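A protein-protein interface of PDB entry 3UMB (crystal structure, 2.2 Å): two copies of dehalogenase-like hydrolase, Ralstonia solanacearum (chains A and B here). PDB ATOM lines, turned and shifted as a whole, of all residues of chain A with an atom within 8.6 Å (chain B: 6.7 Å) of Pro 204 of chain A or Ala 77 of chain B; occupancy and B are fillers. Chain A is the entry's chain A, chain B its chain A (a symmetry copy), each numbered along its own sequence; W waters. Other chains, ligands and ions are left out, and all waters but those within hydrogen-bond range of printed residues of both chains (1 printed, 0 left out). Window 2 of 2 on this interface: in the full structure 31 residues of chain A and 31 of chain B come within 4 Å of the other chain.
The guanidinium group (NH1) of Arg 78 of chain B lies within hydrogen-bond range of the side-chain hydroxyl (OH) of Tyr 74 of chain B, at 3.0 Å.
The guanidinium group (NH1) of Arg 43 of chain B is in hydrogen-bond range of the side-chain hydroxyl (OH) of Tyr 74 of chain B.
The side-chain amide nitrogen (ND2) of Asn 199 of chain A sits at hydrogen-bond distance from the backbone carbonyl oxygen (O) of His 203 of chain A (2.8 Å).
Water W1 lies within hydrogen-bond range of O of Pro 204 of chain A, OH of Tyr 74 of chain B and OE2 of Glu 206 of chain A.
NH1 of Arg 43 of chain B is in salt-bridge range of OE2 of Glu 206 of chain A, at 3.1 Å.
A ring nitrogen (NE2) of His 203 of chain A lies within hydrogen-bond range of the guanidinium group (NE) of Arg 78 of chain B, 3.5 Å away.
No position is printed for both chains.
Of the 8 pairs that touch across the chains among the printed residues, none has its exchanged pair printed and touching as well.
Of the printed residues of chain A, Arg 43 of chain B touches Glu 206.
Printed residues of chain B within 4 Å of His 203 of chain A: Tyr 74 and Arg 78.
Printed residues of chain B within 4 Å of Glu 206 of chain A: Arg 43 and Tyr 74.
Printed residues of chain B within 4 Å of Pro 205 of chain A: Tyr 74.
The nearest residue of chain A that does not touch Ala 77 of chain B is Pro 205 of chain A (6.4 Å).
His 203 of chain A touches Tyr 74 of chain B.
Pro 204 of chain A touches Tyr 74 of chain B (O to CE1, 3.5 Å).
Pro 204 of chain A touches Ala 77 of chain B (CG to C, 3.8 Å).
N of Arg 78 of chain B touches CG of Pro 204 of chain A, at 3.5 Å.
Tyr 74 of chain B touches Pro 205 of chain A.
Glu 206 of chain A touches Tyr 74 of chain B (OE1 to CE1, 3.6 Å).
Hydrophobic or aromatic side chains of chain B that line the printed part of chain A: Tyr 74 and Ala 77.
Among the printed residues, Asp or Glu carboxylates within 4 Å of a Lys or Arg side-chain nitrogen of the other chain: Glu 206 of chain A with Arg 43 of chain B.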
ATOM      1  N   ASN A 181     -16.229 -22.682  -6.598  1.00  0.00           N
ATOM      2  CA  ASN A 181     -17.630 -22.395  -6.467  1.00  0.00           C
ATOM      3  C   ASN A 181     -18.192 -23.544  -5.654  1.00  0.00           C
ATOM      4  O   ASN A 181     -18.077 -24.723  -6.026  1.00  0.00           O
ATOM      5  CB  ASN A 181     -18.245 -22.266  -7.839  1.00  0.00           C
ATOM      6  CG  ASN A 181     -17.754 -21.042  -8.579  1.00  0.00           C
ATOM      7  OD1 ASN A 181     -17.696 -19.984  -8.012  1.00  0.00           O
ATOM      8  ND2 ASN A 181     -17.431 -21.182  -9.852  1.00  0.00           N
ATOM      9  N   GLY A 182     -18.735 -23.209  -4.498  1.00  0.00           N
ATOM     10  CA  GLY A 182     -19.334 -24.218  -3.626  1.00  0.00           C
ATOM     11  C   GLY A 182     -20.340 -25.096  -4.337  1.00  0.00           C
ATOM     12  O   GLY A 182     -20.342 -26.309  -4.138  1.00  0.00           O
ATOM     13  N   TRP A 183     -21.176 -24.505  -5.187  1.00  0.00           N
ATOM     14  CA  TRP A 183     -22.199 -25.293  -5.878  1.00  0.00           C
ATOM     15  C   TRP A 183     -21.533 -26.365  -6.750  1.00  0.00           C
ATOM     16  O   TRP A 183     -22.015 -27.485  -6.871  1.00  0.00           O
ATOM     17  CB  TRP A 183     -23.160 -24.410  -6.690  1.00  0.00           C
ATOM     18  CG  TRP A 183     -22.514 -23.508  -7.727  1.00  0.00           C
ATOM     19  CD1 TRP A 183     -22.174 -22.195  -7.555  1.00  0.00           C
ATOM     20  CD2 TRP A 183     -22.139 -23.846  -9.072  1.00  0.00           C
ATOM     21  NE1 TRP A 183     -21.545 -21.713  -8.689  1.00  0.00           N
ATOM     22  CE2 TRP A 183     -21.552 -22.696  -9.645  1.00  0.00           C
ATOM     23  CE3 TRP A 183     -22.220 -25.013  -9.837  1.00  0.00           C
ATOM     24  CZ2 TRP A 183     -21.087 -22.660 -10.975  1.00  0.00           C
ATOM     25  CZ3 TRP A 183     -21.710 -25.004 -11.153  1.00  0.00           C
ATOM     26  CH2 TRP A 183     -21.147 -23.825 -11.701  1.00  0.00           C
ATOM     27  N   CYS A 186     -19.944 -29.257  -4.826  1.00  0.00           N
ATOM     28  CA  CYS A 186     -21.069 -30.096  -4.399  1.00  0.00           C
ATOM     29  C   CYS A 186     -21.639 -30.935  -5.548  1.00  0.00           C
ATOM     30  O   CYS A 186     -21.972 -32.110  -5.378  1.00  0.00           O
ATOM     31  CB  CYS A 186     -22.171 -29.194  -3.845  1.00  0.00           C
ATOM     32  SG  CYS A 186     -21.824 -28.551  -2.165  1.00  0.00           S
ATOM     33  N   TRP A 197     -12.770 -27.937  -2.308  1.00  0.00           N
ATOM     34  CA  TRP A 197     -13.357 -26.628  -2.514  1.00  0.00           C
ATOM     35  C   TRP A 197     -12.405 -25.523  -2.056  1.00  0.00           C
ATOM     36  O   TRP A 197     -12.131 -25.398  -0.853  1.00  0.00           O
ATOM     37  CB  TRP A 197     -14.685 -26.558  -1.736  1.00  0.00           C
ATOM     38  CG  TRP A 197     -15.395 -25.235  -1.816  1.00  0.00           C
ATOM     39  CD1 TRP A 197     -15.402 -24.356  -2.861  1.00  0.00           C
ATOM     40  CD2 TRP A 197     -16.245 -24.662  -0.809  1.00  0.00           C
ATOM     41  NE1 TRP A 197     -16.189 -23.242  -2.555  1.00  0.00           N
ATOM     42  CE2 TRP A 197     -16.711 -23.417  -1.298  1.00  0.00           C
ATOM     43  CE3 TRP A 197     -16.659 -25.082   0.458  1.00  0.00           C
ATOM     44  CZ2 TRP A 197     -17.558 -22.610  -0.569  1.00  0.00           C
ATOM     45  CZ3 TRP A 197     -17.493 -24.255   1.183  1.00  0.00           C
ATOM     46  CH2 TRP A 197     -17.945 -23.051   0.656  1.00  0.00           C
ATOM     47  N   ASN A 199     -12.486 -22.343  -1.070  1.00  0.00           N
ATOM     48  CA  ASN A 199     -13.422 -21.377  -0.560  1.00  0.00           C
ATOM     49  C   ASN A 199     -12.694 -20.052  -0.244  1.00  0.00           C
ATOM     50  O   ASN A 199     -12.356 -19.756   0.913  1.00  0.00           O
ATOM     51  CB  ASN A 199     -14.108 -21.992   0.687  1.00  0.00           C
ATOM     52  CG  ASN A 199     -15.148 -21.092   1.291  1.00  0.00           C
ATOM     53  OD1 ASN A 199     -15.555 -20.103   0.678  1.00  0.00           O
ATOM     54  ND2 ASN A 199     -15.576 -21.418   2.520  1.00  0.00           N
ATOM     55  N   LEU A 201     -13.572 -16.828  -0.272  1.00  0.00           N
ATOM     56  CA  LEU A 201     -14.214 -15.753   0.461  1.00  0.00           C
ATOM     57  C   LEU A 201     -14.690 -16.206   1.846  1.00  0.00           C
ATOM     58  O   LEU A 201     -15.330 -15.457   2.542  1.00  0.00           O
ATOM     59  CB  LEU A 201     -15.350 -15.171  -0.384  1.00  0.00           C
ATOM     60  CG  LEU A 201     -15.041 -14.613  -1.797  1.00  0.00           C
ATOM     61  CD1 LEU A 201     -16.283 -13.841  -2.344  1.00  0.00           C
ATOM     62  CD2 LEU A 201     -13.789 -13.724  -1.834  1.00  0.00           C
ATOM     63  N   GLY A 202     -14.349 -17.422   2.249  1.00  0.00           N
ATOM     64  CA  GLY A 202     -14.705 -17.933   3.575  1.00  0.00           C
ATOM     65  C   GLY A 202     -16.198 -18.091   3.823  1.00  0.00           C
ATOM     66  O   GLY A 202     -16.670 -17.852   4.906  1.00  0.00           O
ATOM     67  N   HIS A 203     -16.938 -18.526   2.806  1.00  0.00           N
ATOM     68  CA  HIS A 203     -18.388 -18.634   2.901  1.00  0.00           C
ATOM     69  C   HIS A 203     -18.812 -19.922   3.584  1.00  0.00           C
ATOM     70  O   HIS A 203     -17.990 -20.829   3.748  1.00  0.00           O
ATOM     71  CB  HIS A 203     -18.979 -18.541   1.492  1.00  0.00           C
ATOM     72  CG  HIS A 203     -18.970 -17.150   0.940  1.00  0.00           C
ATOM     73  ND1 HIS A 203     -19.190 -16.878  -0.389  1.00  0.00           N
ATOM     74  CD2 HIS A 203     -18.775 -15.952   1.545  1.00  0.00           C
ATOM     75  CE1 HIS A 203     -19.134 -15.573  -0.586  1.00  0.00           C
ATOM     76  NE2 HIS A 203     -18.895 -14.985   0.575  1.00  0.00           N
ATOM     77  N   PRO A 204     -20.091 -20.025   3.993  1.00  0.00           N
ATOM     78  CA  PRO A 204     -20.529 -21.323   4.551  1.00  0.00           C
ATOM     79  C   PRO A 204     -20.643 -22.374   3.457  1.00  0.00           C
ATOM     80  O   PRO A 204     -20.656 -21.997   2.280  1.00  0.00           O
ATOM     81  CB  PRO A 204     -21.890 -21.016   5.174  1.00  0.00           C
ATOM     82  CG  PRO A 204     -22.059 -19.508   5.102  1.00  0.00           C
ATOM     83  CD  PRO A 204     -21.131 -18.993   4.063  1.00  0.00           C
ATOM     84  N   PRO A 205     -20.650 -23.675   3.817  1.00  0.00           N
ATOM     85  CA  PRO A 205     -21.008 -24.660   2.815  1.00  0.00           C
ATOM     86  C   PRO A 205     -22.436 -24.485   2.312  1.00  0.00           C
ATOM     87  O   PRO A 205     -23.314 -24.106   3.046  1.00  0.00           O
ATOM     88  CB  PRO A 205     -20.862 -26.003   3.543  1.00  0.00           C
ATOM     89  CG  PRO A 205     -19.872 -25.752   4.623  1.00  0.00           C
ATOM     90  CD  PRO A 205     -20.116 -24.314   5.044  1.00  0.00           C
ATOM     91  N   GLU A 206     -22.644 -24.775   1.042  1.00  0.00           N
ATOM     92  CA  GLU A 206     -23.980 -24.749   0.462  1.00  0.00           C
ATOM     93  C   GLU A 206     -24.835 -25.780   1.175  1.00  0.00           C
ATOM     94  O   GLU A 206     -24.363 -26.844   1.535  1.00  0.00           O
ATOM     95  CB  GLU A 206     -23.947 -25.030  -1.038  1.00  0.00           C
ATOM     96  CG  GLU A 206     -23.224 -23.997  -1.847  1.00  0.00           C
ATOM     97  CD  GLU A 206     -23.861 -22.599  -1.836  1.00  0.00           C
ATOM     98  OE1 GLU A 206     -24.955 -22.361  -1.317  1.00  0.00           O
ATOM     99  OE2 GLU A 206     -23.248 -21.695  -2.387  1.00  0.00           O
ATOM    100  N   ALA A 207     -26.108 -25.439   1.385  1.00  0.00           N
ATOM    101  CA  ALA A 207     -27.028 -26.334   2.060  1.00  0.00           C
ATOM    102  C   ALA A 207     -27.632 -27.238   0.969  1.00  0.00           C
ATOM    103  O   ALA A 207     -28.750 -27.054   0.548  1.00  0.00           O
ATOM    104  CB  ALA A 207     -28.118 -25.515   2.849  1.00  0.00           C
ATOM    105  N   ALA A 215     -12.110 -28.746   2.003  1.00  0.00           N
ATOM    106  CA  ALA A 215     -12.119 -27.375   1.485  1.00  0.00           C
ATOM    107  C   ALA A 215     -10.959 -26.574   2.148  1.00  0.00           C
ATOM    108  O   ALA A 215     -10.482 -26.929   3.219  1.00  0.00           O
ATOM    109  CB  ALA A 215     -13.468 -26.689   1.784  1.00  0.00           C
ATOM    110  N   ARG B  43     -30.804 -17.872  -3.197  1.00  0.00           N
ATOM    111  CA  ARG B  43     -30.363 -19.264  -2.956  1.00  0.00           C
ATOM    112  C   ARG B  43     -31.502 -20.258  -3.098  1.00  0.00           C
ATOM    113  O   ARG B  43     -31.288 -21.378  -3.538  1.00  0.00           O
ATOM    114  CB  ARG B  43     -29.592 -19.435  -1.632  1.00  0.00           C
ATOM    115  CG  ARG B  43     -28.201 -18.781  -1.704  1.00  0.00           C
ATOM    116  CD  ARG B  43     -27.358 -19.453  -2.786  1.00  0.00           C
ATOM    117  NE  ARG B  43     -25.937 -19.499  -2.455  1.00  0.00           N
ATOM    118  CZ  ARG B  43     -25.046 -18.540  -2.767  1.00  0.00           C
ATOM    119  NH1 ARG B  43     -23.753 -18.683  -2.466  1.00  0.00           N
ATOM    120  NH2 ARG B  43     -25.415 -17.413  -3.377  1.00  0.00           N
ATOM    121  N   LEU B  72     -32.811 -20.648   3.466  1.00  0.00           N
ATOM    122  CA  LEU B  72     -32.935 -19.700   4.572  1.00  0.00           C
ATOM    123  C   LEU B  72     -31.784 -19.881   5.567  1.00  0.00           C
ATOM    124  O   LEU B  72     -31.228 -18.907   6.075  1.00  0.00           O
ATOM    125  CB  LEU B  72     -34.255 -19.920   5.315  1.00  0.00           C
ATOM    126  CG  LEU B  72     -34.416 -19.167   6.654  1.00  0.00           C
ATOM    127  CD1 LEU B  72     -34.507 -17.673   6.333  1.00  0.00           C
ATOM    128  CD2 LEU B  72     -35.612 -19.662   7.419  1.00  0.00           C
ATOM    129  N   ARG B  73     -31.511 -21.144   5.884  1.00  0.00           N
ATOM    130  CA  ARG B  73     -30.364 -21.539   6.683  1.00  0.00           C
ATOM    131  C   ARG B  73     -29.020 -21.115   6.124  1.00  0.00           C
ATOM    132  O   ARG B  73     -28.170 -20.563   6.867  1.00  0.00           O
ATOM    133  CB  ARG B  73     -30.337 -23.037   6.878  1.00  0.00           C
ATOM    134  CG  ARG B  73     -31.430 -23.526   7.811  1.00  0.00           C
ATOM    135  CD  ARG B  73     -31.453 -25.037   7.983  1.00  0.00           C
ATOM    136  NE  ARG B  73     -32.543 -25.418   8.914  1.00  0.00           N
ATOM    137  CZ  ARG B  73     -33.088 -26.633   9.026  1.00  0.00           C
ATOM    138  NH1 ARG B  73     -32.685 -27.646   8.264  1.00  0.00           N
ATOM    139  NH2 ARG B  73     -34.063 -26.836   9.896  1.00  0.00           N
ATOM    140  N   TYR B  74     -28.775 -21.391   4.838  1.00  0.00           N
ATOM    141  CA  TYR B  74     -27.529 -20.898   4.245  1.00  0.00           C
ATOM    142  C   TYR B  74     -27.482 -19.358   4.399  1.00  0.00           C
ATOM    143  O   TYR B  74     -26.452 -18.793   4.802  1.00  0.00           O
ATOM    144  CB  TYR B  74     -27.374 -21.265   2.775  1.00  0.00           C
ATOM    145  CG  TYR B  74     -26.190 -20.574   2.168  1.00  0.00           C
ATOM    146  CD1 TYR B  74     -24.960 -21.200   2.136  1.00  0.00           C
ATOM    147  CD2 TYR B  74     -26.306 -19.312   1.622  1.00  0.00           C
ATOM    148  CE1 TYR B  74     -23.845 -20.588   1.612  1.00  0.00           C
ATOM    149  CE2 TYR B  74     -25.203 -18.664   1.073  1.00  0.00           C
ATOM    150  CZ  TYR B  74     -23.950 -19.326   1.086  1.00  0.00           C
ATOM    151  OH  TYR B  74     -22.810 -18.739   0.577  1.00  0.00           O
ATOM    152  N   ALA B  75     -28.579 -18.680   4.057  1.00  0.00           N
ATOM    153  CA  ALA B  75     -28.544 -17.193   4.024  1.00  0.00           C
ATOM    154  C   ALA B  75     -28.227 -16.626   5.440  1.00  0.00           C
ATOM    155  O   ALA B  75     -27.501 -15.654   5.596  1.00  0.00           O
ATOM    156  CB  ALA B  75     -29.841 -16.645   3.507  1.00  0.00           C
ATOM    157  N   CYS B  76     -28.739 -17.281   6.473  1.00  0.00           N
ATOM    158  CA  CYS B  76     -28.505 -16.788   7.830  1.00  0.00           C
ATOM    159  C   CYS B  76     -27.059 -17.006   8.282  1.00  0.00           C
ATOM    160  O   CYS B  76     -26.499 -16.102   8.863  1.00  0.00           O
ATOM    161  CB  CYS B  76     -29.506 -17.389   8.813  1.00  0.00           C
ATOM    162  SG  CYS B  76     -31.145 -16.586   8.638  1.00  0.00           S
ATOM    163  N   ALA B  77     -26.491 -18.174   7.969  1.00  0.00           N
ATOM    164  CA  ALA B  77     -25.112 -18.527   8.246  1.00  0.00           C
ATOM    165  C   ALA B  77     -24.189 -17.550   7.581  1.00  0.00           C
ATOM    166  O   ALA B  77     -23.305 -17.011   8.230  1.00  0.00           O
ATOM    167  CB  ALA B  77     -24.783 -19.994   7.765  1.00  0.00           C
ATOM    168  N   ARG B  78     -24.429 -17.284   6.300  1.00  0.00           N
ATOM    169  CA  ARG B  78     -23.626 -16.338   5.495  1.00  0.00           C
ATOM    170  C   ARG B  78     -23.681 -14.909   6.028  1.00  0.00           C
ATOM    171  O   ARG B  78     -22.718 -14.178   5.977  1.00  0.00           O
ATOM    172  CB  ARG B  78     -24.125 -16.393   4.049  1.00  0.00           C
ATOM    173  CG  ARG B  78     -23.727 -15.297   3.070  1.00  0.00           C
ATOM    174  CD  ARG B  78     -22.419 -15.574   2.293  1.00  0.00           C
ATOM    175  NE  ARG B  78     -22.289 -14.610   1.187  1.00  0.00           N
ATOM    176  CZ  ARG B  78     -22.687 -14.821  -0.090  1.00  0.00           C
ATOM    177  NH1 ARG B  78     -23.187 -15.989  -0.515  1.00  0.00           N
ATOM    178  NH2 ARG B  78     -22.547 -13.840  -0.973  1.00  0.00           N
ATOM    179  N   LEU B  79     -24.856 -14.508   6.511  1.00  0.00           N
ATOM    180  CA  LEU B  79     -25.116 -13.143   6.896  1.00  0.00           C
ATOM    181  C   LEU B  79     -24.917 -12.991   8.397  1.00  0.00           C
ATOM    182  O   LEU B  79     -25.205 -11.926   8.960  1.00  0.00           O
ATOM    183  CB  LEU B  79     -26.559 -12.757   6.520  1.00  0.00           C
ATOM    184  CG  LEU B  79     -26.896 -12.327   5.083  1.00  0.00           C
ATOM    185  CD1 LEU B  79     -28.384 -12.057   4.975  1.00  0.00           C
ATOM    186  CD2 LEU B  79     -26.055 -11.095   4.679  1.00  0.00           C
ATOM    187  N   ASN B  80     -24.447 -14.052   9.040  1.00  0.00           N
ATOM    188  CA  ASN B  80     -24.155 -14.072  10.488  1.00  0.00           C
ATOM    189  C   ASN B  80     -25.324 -13.713  11.405  1.00  0.00           C
ATOM    190  O   ASN B  80     -25.107 -13.100  12.451  1.00  0.00           O
ATOM    191  CB  ASN B  80     -22.948 -13.173  10.794  1.00  0.00           C
ATOM    192  CG  ASN B  80     -21.695 -13.705  10.179  1.00  0.00           C
ATOM    193  OD1 ASN B  80     -21.433 -14.913  10.273  1.00  0.00           O
ATOM    194  ND2 ASN B  80     -20.903 -12.826   9.544  1.00  0.00           N
ATOM    195  N   LEU B  81     -26.526 -14.174  11.037  1.00  0.00           N
ATOM    196  CA  LEU B  81     -27.764 -13.951  11.792  1.00  0.00           C
ATOM    197  C   LEU B  81     -28.164 -15.101  12.744  1.00  0.00           C
ATOM    198  O   LEU B  81     -28.114 -16.269  12.347  1.00  0.00           O
ATOM    199  CB  LEU B  81     -28.904 -13.714  10.804  1.00  0.00           C
ATOM    200  CG  LEU B  81     -28.663 -12.657   9.733  1.00  0.00           C
ATOM    201  CD1 LEU B  81     -29.889 -12.616   8.782  1.00  0.00           C
ATOM    202  CD2 LEU B  81     -28.405 -11.296  10.356  1.00  0.00           C
ATOM    203  N   LEU B  83     -30.327 -17.468  13.785  1.00  0.00           N
ATOM    204  CA  LEU B  83     -31.493 -18.248  13.380  1.00  0.00           C
ATOM    205  C   LEU B  83     -31.478 -19.622  14.045  1.00  0.00           C
ATOM    206  O   LEU B  83     -30.861 -20.557  13.553  1.00  0.00           O
ATOM    207  CB  LEU B  83     -31.533 -18.417  11.848  1.00  0.00           C
ATOM    208  CG  LEU B  83     -32.731 -19.190  11.263  1.00  0.00           C
ATOM    209  CD1 LEU B  83     -33.775 -18.215  10.687  1.00  0.00           C
ATOM    210  CD2 LEU B  83     -32.267 -20.184  10.211  1.00  0.00           C
HETATM  211  O   HOH W   1     -20.971 -21.086  -0.268  1.00  0.00           O
